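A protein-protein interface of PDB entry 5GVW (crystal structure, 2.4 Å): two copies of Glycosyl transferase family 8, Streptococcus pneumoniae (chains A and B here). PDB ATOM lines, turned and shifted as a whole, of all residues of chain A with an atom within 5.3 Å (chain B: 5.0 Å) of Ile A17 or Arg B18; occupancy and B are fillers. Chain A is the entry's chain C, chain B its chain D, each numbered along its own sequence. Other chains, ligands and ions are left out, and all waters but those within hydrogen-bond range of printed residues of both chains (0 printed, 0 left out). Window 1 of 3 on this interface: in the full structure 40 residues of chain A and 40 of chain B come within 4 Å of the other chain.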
ATOM      1  N   ASP A  13     -15.629 -25.024  19.510  1.00  0.00           N
ATOM      2  CA  ASP A  13     -15.916 -25.463  18.131  1.00  0.00           C
ATOM      3  C   ASP A  13     -16.347 -24.334  17.168  1.00  0.00           C
ATOM      4  O   ASP A  13     -16.365 -23.160  17.542  1.00  0.00           O
ATOM      5  CB  ASP A  13     -16.883 -26.659  18.135  1.00  0.00           C
ATOM      6  CG  ASP A  13     -16.133 -28.018  18.178  1.00  0.00           C
ATOM      7  OD1 ASP A  13     -14.862 -28.010  18.173  1.00  0.00           O
ATOM      8  OD2 ASP A  13     -16.815 -29.088  18.208  1.00  0.00           O
ATOM      9  N   TYR A  14     -16.606 -24.695  15.908  1.00  0.00           N
ATOM     10  CA  TYR A  14     -16.831 -23.723  14.835  1.00  0.00           C
ATOM     11  C   TYR A  14     -18.093 -22.910  15.079  1.00  0.00           C
ATOM     12  O   TYR A  14     -18.073 -21.667  14.885  1.00  0.00           O
ATOM     13  CB  TYR A  14     -16.881 -24.433  13.464  1.00  0.00           C
ATOM     14  CG  TYR A  14     -16.863 -23.570  12.205  1.00  0.00           C
ATOM     15  CD1 TYR A  14     -16.272 -22.304  12.176  1.00  0.00           C
ATOM     16  CD2 TYR A  14     -17.392 -24.061  11.015  1.00  0.00           C
ATOM     17  CE1 TYR A  14     -16.236 -21.552  10.992  1.00  0.00           C
ATOM     18  CE2 TYR A  14     -17.361 -23.325   9.844  1.00  0.00           C
ATOM     19  CZ  TYR A  14     -16.776 -22.079   9.836  1.00  0.00           C
ATOM     20  OH  TYR A  14     -16.737 -21.340   8.681  1.00  0.00           O
ATOM     21  N   ALA A  15     -19.157 -23.605  15.535  1.00  0.00           N
ATOM     22  CA  ALA A  15     -20.459 -22.973  15.862  1.00  0.00           C
ATOM     23  C   ALA A  15     -20.344 -21.730  16.746  1.00  0.00           C
ATOM     24  O   ALA A  15     -21.197 -20.860  16.673  1.00  0.00           O
ATOM     25  CB  ALA A  15     -21.420 -23.975  16.498  1.00  0.00           C
ATOM     26  N   TYR A  16     -19.285 -21.650  17.552  1.00  0.00           N
ATOM     27  CA  TYR A  16     -19.058 -20.521  18.457  1.00  0.00           C
ATOM     28  C   TYR A  16     -17.948 -19.604  17.956  1.00  0.00           C
ATOM     29  O   TYR A  16     -17.347 -18.865  18.734  1.00  0.00           O
ATOM     30  CB  TYR A  16     -18.776 -21.010  19.896  1.00  0.00           C
ATOM     31  CG  TYR A  16     -19.726 -22.122  20.358  1.00  0.00           C
ATOM     32  CD1 TYR A  16     -19.434 -23.471  20.095  1.00  0.00           C
ATOM     33  CD2 TYR A  16     -20.917 -21.829  21.028  1.00  0.00           C
ATOM     34  CE1 TYR A  16     -20.284 -24.490  20.502  1.00  0.00           C
ATOM     35  CE2 TYR A  16     -21.778 -22.843  21.437  1.00  0.00           C
ATOM     36  CZ  TYR A  16     -21.456 -24.167  21.173  1.00  0.00           C
ATOM     37  OH  TYR A  16     -22.303 -25.172  21.567  1.00  0.00           O
ATOM     38  N   ILE A  17     -17.686 -19.619  16.655  1.00  0.00           N
ATOM     39  CA  ILE A  17     -16.525 -18.895  16.139  1.00  0.00           C
ATOM     40  C   ILE A  17     -16.685 -17.399  16.339  1.00  0.00           C
ATOM     41  O   ILE A  17     -15.720 -16.731  16.691  1.00  0.00           O
ATOM     42  CB  ILE A  17     -16.156 -19.274  14.689  1.00  0.00           C
ATOM     43  CG1 ILE A  17     -14.786 -18.672  14.294  1.00  0.00           C
ATOM     44  CG2 ILE A  17     -17.246 -18.861  13.699  1.00  0.00           C
ATOM     45  CD1 ILE A  17     -13.599 -19.374  14.924  1.00  0.00           C
ATOM     46  N   ARG A  18     -17.906 -16.890  16.151  1.00  0.00           N
ATOM     47  CA  ARG A  18     -18.228 -15.473  16.443  1.00  0.00           C
ATOM     48  C   ARG A  18     -17.904 -15.030  17.885  1.00  0.00           C
ATOM     49  O   ARG A  18     -17.361 -13.937  18.077  1.00  0.00           O
ATOM     50  CB  ARG A  18     -19.707 -15.145  16.102  1.00  0.00           C
ATOM     51  CG  ARG A  18     -20.024 -15.181  14.601  1.00  0.00           C
ATOM     52  CD  ARG A  18     -21.435 -14.749  14.274  1.00  0.00           C
ATOM     53  NE  ARG A  18     -21.692 -13.377  14.698  1.00  0.00           N
ATOM     54  CZ  ARG A  18     -22.536 -13.006  15.665  1.00  0.00           C
ATOM     55  NH1 ARG A  18     -23.284 -13.885  16.358  1.00  0.00           N
ATOM     56  NH2 ARG A  18     -22.635 -11.720  15.945  1.00  0.00           N
ATOM     57  N   GLN A  19     -18.191 -15.901  18.861  1.00  0.00           N
ATOM     58  CA  GLN A  19     -17.827 -15.703  20.284  1.00  0.00           C
ATOM     59  C   GLN A  19     -16.297 -15.768  20.476  1.00  0.00           C
ATOM     60  O   GLN A  19     -15.689 -14.859  21.074  1.00  0.00           O
ATOM     61  CB  GLN A  19     -18.507 -16.744  21.198  1.00  0.00           C
ATOM     62  CG  GLN A  19     -20.030 -16.613  21.244  1.00  0.00           C
ATOM     63  CD  GLN A  19     -20.677 -16.862  19.867  1.00  0.00           C
ATOM     64  OE1 GLN A  19     -20.246 -17.753  19.147  1.00  0.00           O
ATOM     65  NE2 GLN A  19     -21.677 -16.046  19.481  1.00  0.00           N
ATOM     66  N   ILE A  20     -15.690 -16.842  19.951  1.00  0.00           N
ATOM     67  CA  ILE A  20     -14.243 -17.056  20.070  1.00  0.00           C
ATOM     68  C   ILE A  20     -13.486 -15.868  19.501  1.00  0.00           C
ATOM     69  O   ILE A  20     -12.650 -15.289  20.207  1.00  0.00           O
ATOM     70  CB  ILE A  20     -13.777 -18.351  19.389  1.00  0.00           C
ATOM     71  CG1 ILE A  20     -14.264 -19.564  20.152  1.00  0.00           C
ATOM     72  CG2 ILE A  20     -12.255 -18.434  19.319  1.00  0.00           C
ATOM     73  CD1 ILE A  20     -14.326 -20.814  19.298  1.00  0.00           C
ATOM     74  N   GLU A  21     -13.785 -15.499  18.251  1.00  0.00           N
ATOM     75  CA  GLU A  21     -13.078 -14.391  17.582  1.00  0.00           C
ATOM     76  C   GLU A  21     -13.249 -13.049  18.344  1.00  0.00           C
ATOM     77  O   GLU A  21     -12.327 -12.220  18.401  1.00  0.00           O
ATOM     78  CB  GLU A  21     -13.510 -14.262  16.096  1.00  0.00           C
ATOM     79  CG  GLU A  21     -12.707 -13.206  15.310  1.00  0.00           C
ATOM     80  CD  GLU A  21     -12.932 -13.202  13.796  1.00  0.00           C
ATOM     81  OE1 GLU A  21     -12.326 -12.334  13.117  1.00  0.00           O
ATOM     82  OE2 GLU A  21     -13.697 -14.057  13.272  1.00  0.00           O
ATOM     83  N   THR A  22     -14.425 -12.835  18.929  1.00  0.00           N
ATOM     84  CA  THR A  22     -14.695 -11.578  19.629  1.00  0.00           C
ATOM     85  C   THR A  22     -13.842 -11.529  20.867  1.00  0.00           C
ATOM     86  O   THR A  22     -13.148 -10.530  21.127  1.00  0.00           O
ATOM     87  CB  THR A  22     -16.184 -11.463  19.991  1.00  0.00           C
ATOM     88  OG1 THR A  22     -16.958 -11.437  18.780  1.00  0.00           O
ATOM     89  CG2 THR A  22     -16.464 -10.186  20.796  1.00  0.00           C
ATOM     90  N   ILE A  43     -12.816 -26.080  13.251  1.00  0.00           N
ATOM     91  CA  ILE A  43     -12.611 -24.703  12.734  1.00  0.00           C
ATOM     92  C   ILE A  43     -11.799 -24.755  11.427  1.00  0.00           C
ATOM     93  O   ILE A  43     -10.675 -25.262  11.415  1.00  0.00           O
ATOM     94  CB  ILE A  43     -11.913 -23.791  13.751  1.00  0.00           C
ATOM     95  CG1 ILE A  43     -12.730 -23.752  15.055  1.00  0.00           C
ATOM     96  CG2 ILE A  43     -11.705 -22.396  13.152  1.00  0.00           C
ATOM     97  CD1 ILE A  43     -12.207 -22.800  16.101  1.00  0.00           C
ATOM     98  N   TRP A  47      -9.395 -19.628   8.399  1.00  0.00           N
ATOM     99  CA  TRP A  47      -9.615 -18.721   9.525  1.00  0.00           C
ATOM    100  C   TRP A  47      -8.353 -18.579  10.349  1.00  0.00           C
ATOM    101  O   TRP A  47      -7.886 -17.458  10.617  1.00  0.00           O
ATOM    102  CB  TRP A  47     -10.780 -19.219  10.403  1.00  0.00           C
ATOM    103  CG  TRP A  47     -11.169 -18.248  11.460  1.00  0.00           C
ATOM    104  CD1 TRP A  47     -12.048 -17.215  11.352  1.00  0.00           C
ATOM    105  CD2 TRP A  47     -10.658 -18.208  12.774  1.00  0.00           C
ATOM    106  NE1 TRP A  47     -12.100 -16.521  12.529  1.00  0.00           N
ATOM    107  CE2 TRP A  47     -11.251 -17.118  13.421  1.00  0.00           C
ATOM    108  CE3 TRP A  47      -9.730 -18.985  13.469  1.00  0.00           C
ATOM    109  CZ2 TRP A  47     -10.971 -16.801  14.737  1.00  0.00           C
ATOM    110  CZ3 TRP A  47      -9.444 -18.665  14.758  1.00  0.00           C
ATOM    111  CH2 TRP A  47     -10.064 -17.583  15.388  1.00  0.00           C
ATOM    112  N   TYR B  16     -27.300 -17.643   9.830  1.00  0.00           N
ATOM    113  CA  TYR B  16     -26.520 -17.395   8.596  1.00  0.00           C
ATOM    114  C   TYR B  16     -25.891 -15.983   8.527  1.00  0.00           C
ATOM    115  O   TYR B  16     -25.563 -15.481   7.442  1.00  0.00           O
ATOM    116  CB  TYR B  16     -27.370 -17.675   7.339  1.00  0.00           C
ATOM    117  CG  TYR B  16     -28.183 -18.935   7.481  1.00  0.00           C
ATOM    118  CD1 TYR B  16     -29.555 -18.870   7.827  1.00  0.00           C
ATOM    119  CD2 TYR B  16     -27.595 -20.201   7.341  1.00  0.00           C
ATOM    120  CE1 TYR B  16     -30.320 -20.015   8.000  1.00  0.00           C
ATOM    121  CE2 TYR B  16     -28.357 -21.357   7.523  1.00  0.00           C
ATOM    122  CZ  TYR B  16     -29.715 -21.249   7.853  1.00  0.00           C
ATOM    123  OH  TYR B  16     -30.484 -22.356   8.043  1.00  0.00           O
ATOM    124  N   ILE B  17     -25.660 -15.351   9.668  1.00  0.00           N
ATOM    125  CA  ILE B  17     -25.129 -14.002   9.623  1.00  0.00           C
ATOM    126  C   ILE B  17     -23.725 -13.955   9.005  1.00  0.00           C
ATOM    127  O   ILE B  17     -23.381 -12.955   8.388  1.00  0.00           O
ATOM    128  CB  ILE B  17     -25.155 -13.297  10.993  1.00  0.00           C
ATOM    129  CG1 ILE B  17     -24.982 -11.778  10.802  1.00  0.00           C
ATOM    130  CG2 ILE B  17     -24.086 -13.861  11.945  1.00  0.00           C
ATOM    131  CD1 ILE B  17     -26.218 -11.057  10.273  1.00  0.00           C
ATOM    132  N   ARG B  18     -22.928 -15.010   9.165  1.00  0.00           N
ATOM    133  CA  ARG B  18     -21.601 -15.066   8.553  1.00  0.00           C
ATOM    134  C   ARG B  18     -21.631 -15.089   7.039  1.00  0.00           C
ATOM    135  O   ARG B  18     -20.814 -14.432   6.422  1.00  0.00           O
ATOM    136  CB  ARG B  18     -20.826 -16.277   9.056  1.00  0.00           C
ATOM    137  CG  ARG B  18     -20.472 -16.107  10.518  1.00  0.00           C
ATOM    138  CD  ARG B  18     -19.517 -17.145  11.054  1.00  0.00           C
ATOM    139  NE  ARG B  18     -18.273 -17.183  10.290  1.00  0.00           N
ATOM    140  CZ  ARG B  18     -17.838 -18.211   9.575  1.00  0.00           C
ATOM    141  NH1 ARG B  18     -18.531 -19.352   9.518  1.00  0.00           N
ATOM    142  NH2 ARG B  18     -16.679 -18.097   8.930  1.00  0.00           N
ATOM    143  N   GLN B  19     -22.594 -15.816   6.467  1.00  0.00           N
ATOM    144  CA  GLN B  19     -22.767 -15.970   5.008  1.00  0.00           C
ATOM    145  C   GLN B  19     -23.306 -14.640   4.438  1.00  0.00           C
ATOM    146  O   GLN B  19     -22.786 -14.077   3.459  1.00  0.00           O
ATOM    147  CB  GLN B  19     -23.778 -17.082   4.703  1.00  0.00           C
ATOM    148  CG  GLN B  19     -23.448 -18.528   5.143  1.00  0.00           C
ATOM    149  CD  GLN B  19     -22.974 -18.683   6.613  1.00  0.00           C
ATOM    150  OE1 GLN B  19     -23.498 -18.035   7.529  1.00  0.00           O
ATOM    151  NE2 GLN B  19     -21.948 -19.516   6.833  1.00  0.00           N
ATOM    152  N   ILE B  20     -24.351 -14.141   5.102  1.00  0.00           N
ATOM    153  CA  ILE B  20     -25.049 -12.909   4.740  1.00  0.00           C
ATOM    154  C   ILE B  20     -24.096 -11.728   4.757  1.00  0.00           C
ATOM    155  O   ILE B  20     -24.043 -10.959   3.817  1.00  0.00           O
ATOM    156  CB  ILE B  20     -26.200 -12.608   5.739  1.00  0.00           C
ATOM    157  CG1 ILE B  20     -27.305 -13.639   5.615  1.00  0.00           C
ATOM    158  CG2 ILE B  20     -26.827 -11.216   5.512  1.00  0.00           C
ATOM    159  CD1 ILE B  20     -28.205 -13.680   6.820  1.00  0.00           C
ATOM    160  N   GLU B  21     -23.391 -11.558   5.868  1.00  0.00           N
ATOM    161  CA  GLU B  21     -22.436 -10.470   5.992  1.00  0.00           C
ATOM    162  C   GLU B  21     -21.413 -10.570   4.872  1.00  0.00           C
ATOM    163  O   GLU B  21     -21.037  -9.558   4.281  1.00  0.00           O
ATOM    164  CB  GLU B  21     -21.776 -10.448   7.376  1.00  0.00           C
ATOM    165  CG  GLU B  21     -20.900  -9.206   7.616  1.00  0.00           C
ATOM    166  CD  GLU B  21     -20.554  -8.947   9.091  1.00  0.00           C
ATOM    167  OE1 GLU B  21     -21.144  -9.618   9.982  1.00  0.00           O
ATOM    168  OE2 GLU B  21     -19.696  -8.044   9.349  1.00  0.00           O
ATOM    169  N   THR B  22     -21.007 -11.787   4.535  1.00  0.00           N
ATOM    170  CA  THR B  22     -19.974 -11.979   3.527  1.00  0.00           C
ATOM    171  C   THR B  22     -20.482 -11.635   2.152  1.00  0.00           C
ATOM    172  O   THR B  22     -19.844 -10.889   1.429  1.00  0.00           O
ATOM    173  CB  THR B  22     -19.461 -13.425   3.558  1.00  0.00           C
ATOM    174  OG1 THR B  22     -19.069 -13.718   4.900  1.00  0.00           O
ATOM    175  CG2 THR B  22     -18.250 -13.628   2.608  1.00  0.00           C
ATOM    176  N   TRP B 235     -17.516 -22.597   3.208  1.00  0.00           N
ATOM    177  CA  TRP B 235     -17.198 -22.201   4.589  1.00  0.00           C
ATOM    178  C   TRP B 235     -17.172 -23.358   5.585  1.00  0.00           C
ATOM    179  O   TRP B 235     -16.702 -23.162   6.686  1.00  0.00           O
ATOM    180  CB  TRP B 235     -18.174 -21.107   5.079  1.00  0.00           C
ATOM    181  CG  TRP B 235     -19.623 -21.528   5.030  1.00  0.00           C
ATOM    182  CD1 TRP B 235     -20.284 -22.359   5.912  1.00  0.00           C
ATOM    183  CD2 TRP B 235     -20.574 -21.161   4.038  1.00  0.00           C
ATOM    184  NE1 TRP B 235     -21.585 -22.514   5.531  1.00  0.00           N
ATOM    185  CE2 TRP B 235     -21.799 -21.789   4.384  1.00  0.00           C
ATOM    186  CE3 TRP B 235     -20.525 -20.349   2.901  1.00  0.00           C
ATOM    187  CZ2 TRP B 235     -22.962 -21.628   3.620  1.00  0.00           C
ATOM    188  CZ3 TRP B 235     -21.680 -20.197   2.151  1.00  0.00           C
ATOM    189  CH2 TRP B 235     -22.878 -20.834   2.516  1.00  0.00           C
ATOM    190  N   TRP B 247     -14.569 -17.401  -1.246  1.00  0.00           N
ATOM    191  CA  TRP B 247     -15.521 -17.098  -0.175  1.00  0.00           C
ATOM    192  C   TRP B 247     -14.758 -16.537   1.025  1.00  0.00           C
ATOM    193  O   TRP B 247     -15.160 -15.525   1.624  1.00  0.00           O
ATOM    194  CB  TRP B 247     -16.344 -18.328   0.240  1.00  0.00           C
ATOM    195  CG  TRP B 247     -17.387 -17.964   1.235  1.00  0.00           C
ATOM    196  CD1 TRP B 247     -18.665 -17.590   0.969  1.00  0.00           C
ATOM    197  CD2 TRP B 247     -17.246 -17.915   2.660  1.00  0.00           C
ATOM    198  NE1 TRP B 247     -19.343 -17.318   2.138  1.00  0.00           N
ATOM    199  CE2 TRP B 247     -18.489 -17.502   3.192  1.00  0.00           C
ATOM    200  CE3 TRP B 247     -16.191 -18.178   3.544  1.00  0.00           C
ATOM    201  CZ2 TRP B 247     -18.701 -17.330   4.574  1.00  0.00           C
ATOM    202  CZ3 TRP B 247     -16.405 -18.009   4.933  1.00  0.00           C
ATOM    203  CH2 TRP B 247     -17.651 -17.583   5.424  1.00  0.00           C
ATOM    204  N   TRP B 248     -13.642 -17.203   1.343  1.00  0.00           N
ATOM    205  CA  TRP B 248     -12.783 -16.819   2.466  1.00  0.00           C
ATOM    206  C   TRP B 248     -12.106 -15.447   2.280  1.00  0.00           C
ATOM    207  O   TRP B 248     -11.898 -14.750   3.266  1.00  0.00           O
ATOM    208  CB  TRP B 248     -11.779 -17.951   2.822  1.00  0.00           C
ATOM    209  CG  TRP B 248     -12.477 -19.126   3.441  1.00  0.00           C
ATOM    210  CD1 TRP B 248     -12.917 -20.223   2.807  1.00  0.00           C
ATOM    211  CD2 TRP B 248     -12.862 -19.283   4.812  1.00  0.00           C
ATOM    212  NE1 TRP B 248     -13.548 -21.084   3.685  1.00  0.00           N
ATOM    213  CE2 TRP B 248     -13.538 -20.518   4.923  1.00  0.00           C
ATOM    214  CE3 TRP B 248     -12.710 -18.497   5.956  1.00  0.00           C
ATOM    215  CZ2 TRP B 248     -14.049 -20.988   6.121  1.00  0.00           C
ATOM    216  CZ3 TRP B 248     -13.219 -18.968   7.149  1.00  0.00           C
ATOM    217  CH2 TRP B 248     -13.890 -20.201   7.217  1.00  0.00           C
ATOM    218  N   SER B 251     -15.095 -13.146   3.349  1.00  0.00           N
ATOM    219  CA  SER B 251     -15.441 -13.434   4.750  1.00  0.00           C
ATOM    220  C   SER B 251     -14.466 -12.843   5.745  1.00  0.00           C
ATOM    221  O   SER B 251     -14.890 -12.287   6.752  1.00  0.00           O
ATOM    222  CB  SER B 251     -15.515 -14.935   4.983  1.00  0.00           C
ATOM    223  OG  SER B 251     -15.557 -15.240   6.363  1.00  0.00           O
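OH of Tyr A14 is in hydrogen-bond range of NH1 of Arg B18 (2.8 Å).
O of Trp B235 sits at hydrogen-bond distance from OH of Tyr A14 (2.7 Å).
O of Arg A18 is in hydrogen-bond range of OG1 of Thr A22.
OG1 of Thr B22 sits at hydrogen-bond distance from O of Arg B18 (2.4 Å).
NE2 of Gln B19 lies close to NE1 of Trp B235.
Among the printed residues, merely in contact across the chains: Tyr A14 with Trp B248 (3.4 Å), Arg A18 with Ile B17 (3.6 Å) and Ile A17 with Arg B18 (3.9 Å).
Of the printed residues of chain A, Ile B17 touches Arg A18.
Printed residues of chain B within 4 Å of Tyr A14: Arg B18, Trp B235 and Trp B248.
Printed residues of chain A within 4 Å of Trp B235: Tyr A14 (2.7 Å).
Printed residues of chain B within 4 Å of Arg A18: Ile B17 (3.6 Å).
Gln A19 touches none of the printed residues of chain B.
The nearest printed residue of chain B that does not touch Ile A17 is Trp B248 (7.3 Å).
The nearest residue of chain A that does not touch Arg B18 is Arg A18 (4.1 Å).
Of the 12 printed residues of chain A, 3 touch a printed residue of chain B.
Hydrophobic or aromatic side chains of chain A that line the printed part of chain B: Tyr A14 and Ile A17.
Of the 11 printed residues of chain B, 4 touch a printed residue of chain A.
Among the printed residues, 5 pairs touch across the chains.
Ile A17 touches Arg B18, and with the chains exchanged Arg A18 touches Ile B17.
7 positions are printed for both chains.
Of the 5 pairs that touch across the chains among the printed residues, 2 have their exchanged pair printed and touching as well.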
